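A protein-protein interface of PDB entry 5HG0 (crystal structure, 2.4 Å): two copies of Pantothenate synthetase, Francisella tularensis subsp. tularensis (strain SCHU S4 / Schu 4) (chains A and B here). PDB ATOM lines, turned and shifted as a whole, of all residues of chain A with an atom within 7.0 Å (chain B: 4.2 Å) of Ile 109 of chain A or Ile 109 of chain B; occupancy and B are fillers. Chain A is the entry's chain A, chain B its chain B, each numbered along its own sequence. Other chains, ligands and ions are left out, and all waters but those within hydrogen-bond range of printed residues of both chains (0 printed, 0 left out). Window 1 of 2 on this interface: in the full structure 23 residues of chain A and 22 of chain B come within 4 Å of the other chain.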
ATOM      1  N   ASN A 105     -35.772   9.132  14.798  1.00  0.00           N
ATOM      2  CA  ASN A 105     -34.430   9.608  14.467  1.00  0.00           C
ATOM      3  C   ASN A 105     -34.277  11.058  14.928  1.00  0.00           C
ATOM      4  O   ASN A 105     -34.192  12.000  14.137  1.00  0.00           O
ATOM      5  CB  ASN A 105     -34.171   9.452  12.972  1.00  0.00           C
ATOM      6  CG  ASN A 105     -32.746   9.793  12.589  1.00  0.00           C
ATOM      7  OD1 ASN A 105     -32.497  10.358  11.524  1.00  0.00           O
ATOM      8  ND2 ASN A 105     -31.802   9.462  13.461  1.00  0.00           N
ATOM      9  N   LEU A 106     -34.222  11.216  16.251  1.00  0.00           N
ATOM     10  CA  LEU A 106     -34.256  12.533  16.876  1.00  0.00           C
ATOM     11  C   LEU A 106     -32.870  13.144  17.059  1.00  0.00           C
ATOM     12  O   LEU A 106     -32.685  14.335  16.795  1.00  0.00           O
ATOM     13  CB  LEU A 106     -34.964  12.446  18.231  1.00  0.00           C
ATOM     14  CG  LEU A 106     -36.375  11.855  18.215  1.00  0.00           C
ATOM     15  CD1 LEU A 106     -36.950  11.810  19.620  1.00  0.00           C
ATOM     16  CD2 LEU A 106     -37.286  12.641  17.280  1.00  0.00           C
ATOM     17  N   LEU A 107     -31.894  12.359  17.515  1.00  0.00           N
ATOM     18  CA  LEU A 107     -30.536  12.842  17.760  1.00  0.00           C
ATOM     19  C   LEU A 107     -29.608  12.221  16.723  1.00  0.00           C
ATOM     20  O   LEU A 107     -29.420  11.000  16.703  1.00  0.00           O
ATOM     21  CB  LEU A 107     -30.080  12.503  19.177  1.00  0.00           C
ATOM     22  CG  LEU A 107     -30.898  13.132  20.305  1.00  0.00           C
ATOM     23  CD1 LEU A 107     -30.395  12.660  21.646  1.00  0.00           C
ATOM     24  CD2 LEU A 107     -30.856  14.648  20.223  1.00  0.00           C
ATOM     25  N   ARG A 108     -29.019  13.060  15.877  1.00  0.00           N
ATOM     26  CA  ARG A 108     -28.252  12.605  14.727  1.00  0.00           C
ATOM     27  C   ARG A 108     -26.824  13.122  14.800  1.00  0.00           C
ATOM     28  O   ARG A 108     -26.584  14.256  15.227  1.00  0.00           O
ATOM     29  CB  ARG A 108     -28.904  13.074  13.423  1.00  0.00           C
ATOM     30  CG  ARG A 108     -30.410  12.930  13.426  1.00  0.00           C
ATOM     31  CD  ARG A 108     -31.045  13.628  12.241  1.00  0.00           C
ATOM     32  NE  ARG A 108     -32.501  13.551  12.307  1.00  0.00           N
ATOM     33  CZ  ARG A 108     -33.318  13.876  11.311  1.00  0.00           C
ATOM     34  NH1 ARG A 108     -32.822  14.301  10.155  1.00  0.00           N
ATOM     35  NH2 ARG A 108     -34.630  13.770  11.470  1.00  0.00           N
ATOM     36  N   ILE A 109     -25.879  12.277  14.393  1.00  0.00           N
ATOM     37  CA  ILE A 109     -24.507  12.721  14.177  1.00  0.00           C
ATOM     38  C   ILE A 109     -24.459  13.508  12.874  1.00  0.00           C
ATOM     39  O   ILE A 109     -24.855  13.005  11.817  1.00  0.00           O
ATOM     40  CB  ILE A 109     -23.541  11.530  14.137  1.00  0.00           C
ATOM     41  CG1 ILE A 109     -23.435  10.869  15.513  1.00  0.00           C
ATOM     42  CG2 ILE A 109     -22.173  11.973  13.630  1.00  0.00           C
ATOM     43  CD1 ILE A 109     -22.383  11.484  16.408  1.00  0.00           C
ATOM     44  N   GLU A 110     -23.981  14.747  12.944  1.00  0.00           N
ATOM     45  CA  GLU A 110     -23.840  15.567  11.750  1.00  0.00           C
ATOM     46  C   GLU A 110     -22.367  15.713  11.415  1.00  0.00           C
ATOM     47  O   GLU A 110     -21.593  16.187  12.259  1.00  0.00           O
ATOM     48  CB  GLU A 110     -24.478  16.939  11.952  1.00  0.00           C
ATOM     49  CG  GLU A 110     -25.055  17.538  10.682  1.00  0.00           C
ATOM     50  CD  GLU A 110     -26.269  16.772  10.180  1.00  0.00           C
ATOM     51  OE1 GLU A 110     -27.213  16.566  10.974  1.00  0.00           O
ATOM     52  OE2 GLU A 110     -26.273  16.366   8.996  1.00  0.00           O
ATOM     53  N   PRO A 111     -21.928  15.318  10.223  1.00  0.00           N
ATOM     54  CA  PRO A 111     -20.524  15.524   9.856  1.00  0.00           C
ATOM     55  C   PRO A 111     -20.293  16.873   9.196  1.00  0.00           C
ATOM     56  O   PRO A 111     -20.739  17.109   8.070  1.00  0.00           O
ATOM     57  CB  PRO A 111     -20.239  14.365   8.891  1.00  0.00           C
ATOM     58  CG  PRO A 111     -21.599  13.935   8.363  1.00  0.00           C
ATOM     59  CD  PRO A 111     -22.682  14.646   9.153  1.00  0.00           C
ATOM     60  N   GLY A 126     -27.411  13.358   3.406  1.00  0.00           N
ATOM     61  CA  GLY A 126     -27.928  12.743   4.609  1.00  0.00           C
ATOM     62  C   GLY A 126     -27.466  11.327   4.865  1.00  0.00           C
ATOM     63  O   GLY A 126     -27.663  10.824   5.979  1.00  0.00           O
ATOM     64  N   PHE A 128     -24.361   9.997   5.094  1.00  0.00           N
ATOM     65  CA  PHE A 128     -23.271   9.896   6.059  1.00  0.00           C
ATOM     66  C   PHE A 128     -23.758  10.162   7.476  1.00  0.00           C
ATOM     67  O   PHE A 128     -23.306   9.513   8.427  1.00  0.00           O
ATOM     68  CB  PHE A 128     -22.146  10.857   5.682  1.00  0.00           C
ATOM     69  CG  PHE A 128     -21.261  10.353   4.578  1.00  0.00           C
ATOM     70  CD1 PHE A 128     -21.153   8.995   4.321  1.00  0.00           C
ATOM     71  CD2 PHE A 128     -20.535  11.238   3.800  1.00  0.00           C
ATOM     72  CE1 PHE A 128     -20.335   8.532   3.306  1.00  0.00           C
ATOM     73  CE2 PHE A 128     -19.715  10.781   2.786  1.00  0.00           C
ATOM     74  CZ  PHE A 128     -19.616   9.427   2.537  1.00  0.00           C
ATOM     75  N   SER A 129     -24.682  11.113   7.641  1.00  0.00           N
ATOM     76  CA  SER A 129     -25.254  11.364   8.960  1.00  0.00           C
ATOM     77  C   SER A 129     -26.049  10.163   9.451  1.00  0.00           C
ATOM     78  O   SER A 129     -26.030   9.842  10.645  1.00  0.00           O
ATOM     79  CB  SER A 129     -26.135  12.611   8.923  1.00  0.00           C
ATOM     80  OG  SER A 129     -26.854  12.755  10.137  1.00  0.00           O
ATOM     81  N   GLY A 130     -26.755   9.484   8.546  1.00  0.00           N
ATOM     82  CA  GLY A 130     -27.474   8.287   8.940  1.00  0.00           C
ATOM     83  C   GLY A 130     -26.544   7.138   9.273  1.00  0.00           C
ATOM     84  O   GLY A 130     -26.783   6.391  10.225  1.00  0.00           O
ATOM     85  N   MET A 131     -25.469   6.989   8.506  1.00  0.00           N
ATOM     86  CA  MET A 131     -24.511   5.909   8.715  1.00  0.00           C
ATOM     87  C   MET A 131     -23.776   6.066  10.043  1.00  0.00           C
ATOM     88  O   MET A 131     -23.689   5.121  10.824  1.00  0.00           O
ATOM     89  CB  MET A 131     -23.509   5.857   7.558  1.00  0.00           C
ATOM     90  CG  MET A 131     -22.478   4.740   7.662  1.00  0.00           C
ATOM     91  SD  MET A 131     -20.878   5.232   8.670  1.00  0.00           S
ATOM     92  CE  MET A 131     -20.220   6.652   7.502  1.00  0.00           C
ATOM     93  N   LEU A 132     -23.251   7.269  10.292  1.00  0.00           N
ATOM     94  CA  LEU A 132     -22.489   7.498  11.515  1.00  0.00           C
ATOM     95  C   LEU A 132     -23.361   7.370  12.755  1.00  0.00           C
ATOM     96  O   LEU A 132     -22.880   6.941  13.811  1.00  0.00           O
ATOM     97  CB  LEU A 132     -21.827   8.875  11.470  1.00  0.00           C
ATOM     98  CG  LEU A 132     -20.685   9.030  10.465  1.00  0.00           C
ATOM     99  CD1 LEU A 132     -20.265  10.484  10.347  1.00  0.00           C
ATOM    100  CD2 LEU A 132     -19.506   8.157  10.871  1.00  0.00           C
ATOM    101  N   THR A 133     -24.640   7.738  12.653  1.00  0.00           N
ATOM    102  CA  THR A 133     -25.536   7.624  13.798  1.00  0.00           C
ATOM    103  C   THR A 133     -25.757   6.163  14.174  1.00  0.00           C
ATOM    104  O   THR A 133     -25.645   5.790  15.348  1.00  0.00           O
ATOM    105  CB  THR A 133     -26.871   8.310  13.499  1.00  0.00           C
ATOM    106  OG1 THR A 133     -26.655   9.705  13.248  1.00  0.00           O
ATOM    107  CG2 THR A 133     -27.826   8.158  14.677  1.00  0.00           C
ATOM    108  N   VAL A 134     -26.073   5.319  13.189  1.00  0.00           N
ATOM    109  CA  VAL A 134     -26.325   3.916  13.495  1.00  0.00           C
ATOM    110  C   VAL A 134     -25.034   3.204  13.884  1.00  0.00           C
ATOM    111  O   VAL A 134     -25.053   2.297  14.722  1.00  0.00           O
ATOM    112  CB  VAL A 134     -27.034   3.220  12.317  1.00  0.00           C
ATOM    113  CG1 VAL A 134     -26.055   2.884  11.191  1.00  0.00           C
ATOM    114  CG2 VAL A 134     -27.757   1.971  12.799  1.00  0.00           C
ATOM    115  N   LEU A 136     -22.467   4.542  15.519  1.00  0.00           N
ATOM    116  CA  LEU A 136     -22.262   4.898  16.918  1.00  0.00           C
ATOM    117  C   LEU A 136     -23.179   4.086  17.825  1.00  0.00           C
ATOM    118  O   LEU A 136     -22.740   3.550  18.849  1.00  0.00           O
ATOM    119  CB  LEU A 136     -22.484   6.397  17.116  1.00  0.00           C
ATOM    120  CG  LEU A 136     -22.258   6.943  18.527  1.00  0.00           C
ATOM    121  CD1 LEU A 136     -20.893   6.540  19.042  1.00  0.00           C
ATOM    122  CD2 LEU A 136     -22.399   8.460  18.543  1.00  0.00           C
ATOM    123  N   LEU A 163     -15.009   9.015  13.950  1.00  0.00           N
ATOM    124  CA  LEU A 163     -16.048   8.796  14.952  1.00  0.00           C
ATOM    125  C   LEU A 163     -15.497   8.081  16.177  1.00  0.00           C
ATOM    126  O   LEU A 163     -15.790   8.464  17.316  1.00  0.00           O
ATOM    127  CB  LEU A 163     -17.196   7.993  14.340  1.00  0.00           C
ATOM    128  CG  LEU A 163     -18.406   7.721  15.238  1.00  0.00           C
ATOM    129  CD1 LEU A 163     -19.362   8.908  15.253  1.00  0.00           C
ATOM    130  CD2 LEU A 163     -19.118   6.454  14.800  1.00  0.00           C
ATOM    131  N   PHE A 167     -15.297  10.291  19.919  1.00  0.00           N
ATOM    132  CA  PHE A 167     -16.130   9.894  21.045  1.00  0.00           C
ATOM    133  C   PHE A 167     -15.497   8.777  21.866  1.00  0.00           C
ATOM    134  O   PHE A 167     -16.205   8.051  22.573  1.00  0.00           O
ATOM    135  CB  PHE A 167     -17.522   9.509  20.553  1.00  0.00           C
ATOM    136  CG  PHE A 167     -18.236  10.637  19.871  1.00  0.00           C
ATOM    137  CD1 PHE A 167     -18.701  11.717  20.602  1.00  0.00           C
ATOM    138  CD2 PHE A 167     -18.416  10.636  18.498  1.00  0.00           C
ATOM    139  CE1 PHE A 167     -19.345  12.769  19.977  1.00  0.00           C
ATOM    140  CE2 PHE A 167     -19.062  11.683  17.868  1.00  0.00           C
ATOM    141  CZ  PHE A 167     -19.525  12.753  18.608  1.00  0.00           C
ATOM    142  N   ARG B 108     -20.853  16.328  15.163  1.00  0.00           N
ATOM    143  CA  ARG B 108     -21.706  17.044  16.096  1.00  0.00           C
ATOM    144  C   ARG B 108     -23.020  16.302  16.288  1.00  0.00           C
ATOM    145  O   ARG B 108     -23.561  15.720  15.343  1.00  0.00           O
ATOM    146  CB  ARG B 108     -21.988  18.467  15.600  1.00  0.00           C
ATOM    147  CG  ARG B 108     -20.768  19.179  15.049  1.00  0.00           C
ATOM    148  CD  ARG B 108     -21.117  20.572  14.559  1.00  0.00           C
ATOM    149  NE  ARG B 108     -19.969  21.232  13.943  1.00  0.00           N
ATOM    150  CZ  ARG B 108     -19.950  22.506  13.566  1.00  0.00           C
ATOM    151  NH1 ARG B 108     -21.020  23.269  13.746  1.00  0.00           N
ATOM    152  NH2 ARG B 108     -18.859  23.019  13.011  1.00  0.00           N
ATOM    153  N   ILE B 109     -23.524  16.330  17.517  1.00  0.00           N
ATOM    154  CA  ILE B 109     -24.861  15.832  17.813  1.00  0.00           C
ATOM    155  C   ILE B 109     -25.864  16.914  17.434  1.00  0.00           C
ATOM    156  O   ILE B 109     -25.801  18.037  17.943  1.00  0.00           O
ATOM    157  CB  ILE B 109     -24.997  15.450  19.293  1.00  0.00           C
ATOM    158  CG1 ILE B 109     -23.993  14.355  19.660  1.00  0.00           C
ATOM    159  CG2 ILE B 109     -26.417  15.007  19.600  1.00  0.00           C
ATOM    160  CD1 ILE B 109     -24.263  13.038  18.983  1.00  0.00           C
ATOM    161  N   GLU B 110     -26.787  16.582  16.535  1.00  0.00           N
ATOM    162  CA  GLU B 110     -27.801  17.531  16.101  1.00  0.00           C
ATOM    163  C   GLU B 110     -29.160  17.116  16.639  1.00  0.00           C
ATOM    164  O   GLU B 110     -29.609  15.990  16.376  1.00  0.00           O
ATOM    165  CB  GLU B 110     -27.840  17.630  14.578  1.00  0.00           C
ATOM    166  CG  GLU B 110     -26.831  18.602  13.985  1.00  0.00           C
ATOM    167  CD  GLU B 110     -27.120  20.053  14.337  1.00  0.00           C
ATOM    168  OE1 GLU B 110     -26.211  20.895  14.175  1.00  0.00           O
ATOM    169  OE2 GLU B 110     -28.253  20.354  14.770  1.00  0.00           O
ATOM    170  N   PRO B 111     -29.840  17.975  17.395  1.00  0.00           N
ATOM    171  CA  PRO B 111     -31.183  17.632  17.876  1.00  0.00           C
ATOM    172  C   PRO B 111     -32.277  18.016  16.891  1.00  0.00           C
ATOM    173  O   PRO B 111     -32.470  19.200  16.594  1.00  0.00           O
ATOM    174  CB  PRO B 111     -31.291  18.428  19.181  1.00  0.00           C
ATOM    175  CG  PRO B 111     -30.440  19.638  18.939  1.00  0.00           C
ATOM    176  CD  PRO B 111     -29.329  19.216  18.006  1.00  0.00           C
ATOM    177  N   SER B 129     -26.692  21.775  20.270  1.00  0.00           N
ATOM    178  CA  SER B 129     -25.775  20.890  19.558  1.00  0.00           C
ATOM    179  C   SER B 129     -24.408  20.858  20.227  1.00  0.00           C
ATOM    180  O   SER B 129     -23.817  19.783  20.387  1.00  0.00           O
ATOM    181  CB  SER B 129     -25.644  21.324  18.098  1.00  0.00           C
ATOM    182  OG  SER B 129     -24.642  20.572  17.435  1.00  0.00           O
ATOM    183  N   LEU B 132     -24.830  18.982  23.719  1.00  0.00           N
ATOM    184  CA  LEU B 132     -25.022  17.541  23.591  1.00  0.00           C
ATOM    185  C   LEU B 132     -23.742  16.848  23.145  1.00  0.00           C
ATOM    186  O   LEU B 132     -23.430  15.747  23.614  1.00  0.00           O
ATOM    187  CB  LEU B 132     -26.159  17.247  22.613  1.00  0.00           C
ATOM    188  CG  LEU B 132     -27.564  17.538  23.138  1.00  0.00           C
ATOM    189  CD1 LEU B 132     -28.607  17.319  22.056  1.00  0.00           C
ATOM    190  CD2 LEU B 132     -27.850  16.669  24.349  1.00  0.00           C
ATOM    191  N   THR B 133     -22.988  17.474  22.238  1.00  0.00           N
ATOM    192  CA  THR B 133     -21.755  16.860  21.756  1.00  0.00           C
ATOM    193  C   THR B 133     -20.740  16.695  22.882  1.00  0.00           C
ATOM    194  O   THR B 133     -20.100  15.644  23.001  1.00  0.00           O
ATOM    195  CB  THR B 133     -21.161  17.688  20.617  1.00  0.00           C
ATOM    196  OG1 THR B 133     -22.130  17.837  19.570  1.00  0.00           O
ATOM    197  CG2 THR B 133     -19.919  17.010  20.052  1.00  0.00           C
ATOM    198  N   LEU B 136     -21.801  14.010  25.544  1.00  0.00           N
ATOM    199  CA  LEU B 136     -21.496  12.677  25.037  1.00  0.00           C
ATOM    200  C   LEU B 136     -20.009  12.373  25.173  1.00  0.00           C
ATOM    201  O   LEU B 136     -19.627  11.293  25.636  1.00  0.00           O
ATOM    202  CB  LEU B 136     -21.949  12.555  23.583  1.00  0.00           C
ATOM    203  CG  LEU B 136     -21.738  11.187  22.929  1.00  0.00           C
ATOM    204  CD1 LEU B 136     -22.375  10.085  23.764  1.00  0.00           C
ATOM    205  CD2 LEU B 136     -22.284  11.176  21.505  1.00  0.00           C
ATOM    206  N   PHE B 167     -28.190   6.580  22.650  1.00  0.00           N
ATOM    207  CA  PHE B 167     -26.858   6.038  22.418  1.00  0.00           C
ATOM    208  C   PHE B 167     -26.445   5.041  23.494  1.00  0.00           C
ATOM    209  O   PHE B 167     -25.252   4.783  23.676  1.00  0.00           O
ATOM    210  CB  PHE B 167     -25.849   7.176  22.286  1.00  0.00           C
ATOM    211  CG  PHE B 167     -26.091   8.039  21.083  1.00  0.00           C
ATOM    212  CD1 PHE B 167     -25.799   7.570  19.810  1.00  0.00           C
ATOM    213  CD2 PHE B 167     -26.633   9.307  21.218  1.00  0.00           C
ATOM    214  CE1 PHE B 167     -26.031   8.353  18.695  1.00  0.00           C
ATOM    215  CE2 PHE B 167     -26.867  10.098  20.108  1.00  0.00           C
ATOM    216  CZ  PHE B 167     -26.565   9.621  18.844  1.00  0.00           C
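The backbone NH (N) of Glu 110 of chain B lies within hydrogen-bond range of the backbone carbonyl oxygen (O) of Arg 108 of chain A (2.7 Å).
The backbone NH (N) of Glu 110 of chain A lies within hydrogen-bond range of the backbone carbonyl oxygen (O) of Arg 108 of chain B, at 2.6 Å.
The backbone carbonyl oxygen of Arg 108 of chain A sits close to the backbone carbonyl oxygen of Arg 108 of chain B, at 3.4 Å.
The guanidinium group of Arg 108 of chain A sits at hydrogen-bond distance from the backbone carbonyl oxygen of Asn 105 of chain A, at 2.9 Å.
The backbone carbonyl oxygen (O) of Ile 109 of chain A sits at hydrogen-bond distance from the side-chain hydroxyl (OG) of Ser 129 of chain A (2.6 Å).
The backbone NH of Ile 109 of chain A lies within hydrogen-bond range of the side-chain hydroxyl of Thr 133 of chain A.
The backbone carbonyl oxygen (O) of Ile 109 of chain B is in hydrogen-bond range of the side-chain hydroxyl (OG) of Ser 129 of chain B (2.8 Å).
N of Ile 109 of chain B sits at hydrogen-bond distance from OG1 of Thr 133 of chain B (2.9 Å).
O of Leu 106 of chain A touches C of Pro 111 of chain B, at 3.7 Å.
O of Glu 110 of chain B touches CA of Leu 107 of chain A, at 3.6 Å.
Leu 107 of chain A touches Pro 111 of chain B.
Leu 107 of chain A touches Leu 132 of chain B.
Leu 107 of chain A touches Phe 167 of chain B (O to CZ, 3.8 Å).
CA of Ile 109 of chain B touches O of Arg 108 of chain A (3.5 Å).
CA of Ile 109 of chain A touches O of Arg 108 of chain B, at 3.4 Å.
Ile 109 of chain A touches Ile 109 of chain B (CD1 to CD1, 3.5 Å).
CE1 of Phe 167 of chain B touches CD2 of Leu 136 of chain A (3.6 Å).
Phe 167 of chain A touches Leu 136 of chain B (CE1 to CD2, 3.7 Å).
Of the printed residues of chain B, Leu 107 of chain A touches Glu 110 (3.6 Å), Pro 111 (3.8 Å), Leu 132 (3.9 Å) and Phe 167 (3.8 Å).
Of the printed residues of chain B, Arg 108 of chain A touches Arg 108, Ile 109 and Glu 110.
Ile 109 of chain A touches just these residues of chain B: Arg 108 and Ile 109.
Of the printed residues of chain B, Glu 110 of chain A touches Arg 108 (2.6 Å) and Glu 110 (3.5 Å).
Ser 129 of chain A touches none of the printed residues of chain B.
Printed residues of chain A within 4 Å of Ile 109 of chain B: Arg 108 and Ile 109.
Printed residues of chain A within 4 Å of Pro 111 of chain B: Leu 106 (3.7 Å) and Leu 107 (3.8 Å).
The nearest printed residue of chain B that does not touch Ile 109 of chain A is Phe 167 of chain B (4.7 Å).
Hydrophobic or aromatic side chains of chain B that line the printed part of chain A: Ile 109, Pro 111, Leu 132, Leu 136 and Phe 167.
Of the 18 printed residues of chain A, 7 touch a printed residue of chain B.
Hydrophobic or aromatic side chains of chain A that line the printed part of chain B: Leu 107, Ile 109, Leu 136 and Phe 167.
Among the printed residues, no Asp or Glu carboxylate lies within 4 Å of a Lys or Arg side-chain nitrogen of the other chain.
Arg 108 of chain B touches its own counterpart, Arg 108 of chain A.
Arg 108 of chain A touches Ile 109 of chain B, and with the chains exchanged Ile 109 of chain A touches Arg 108 of chain B.
Arg 108 of chain A touches Glu 110 of chain B, and with the chains exchanged Glu 110 of chain A touches Arg 108 of chain B.
Ile 109 of chain A touches its own counterpart, Ile 109 of chain B.
9 positions are printed for both chains.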
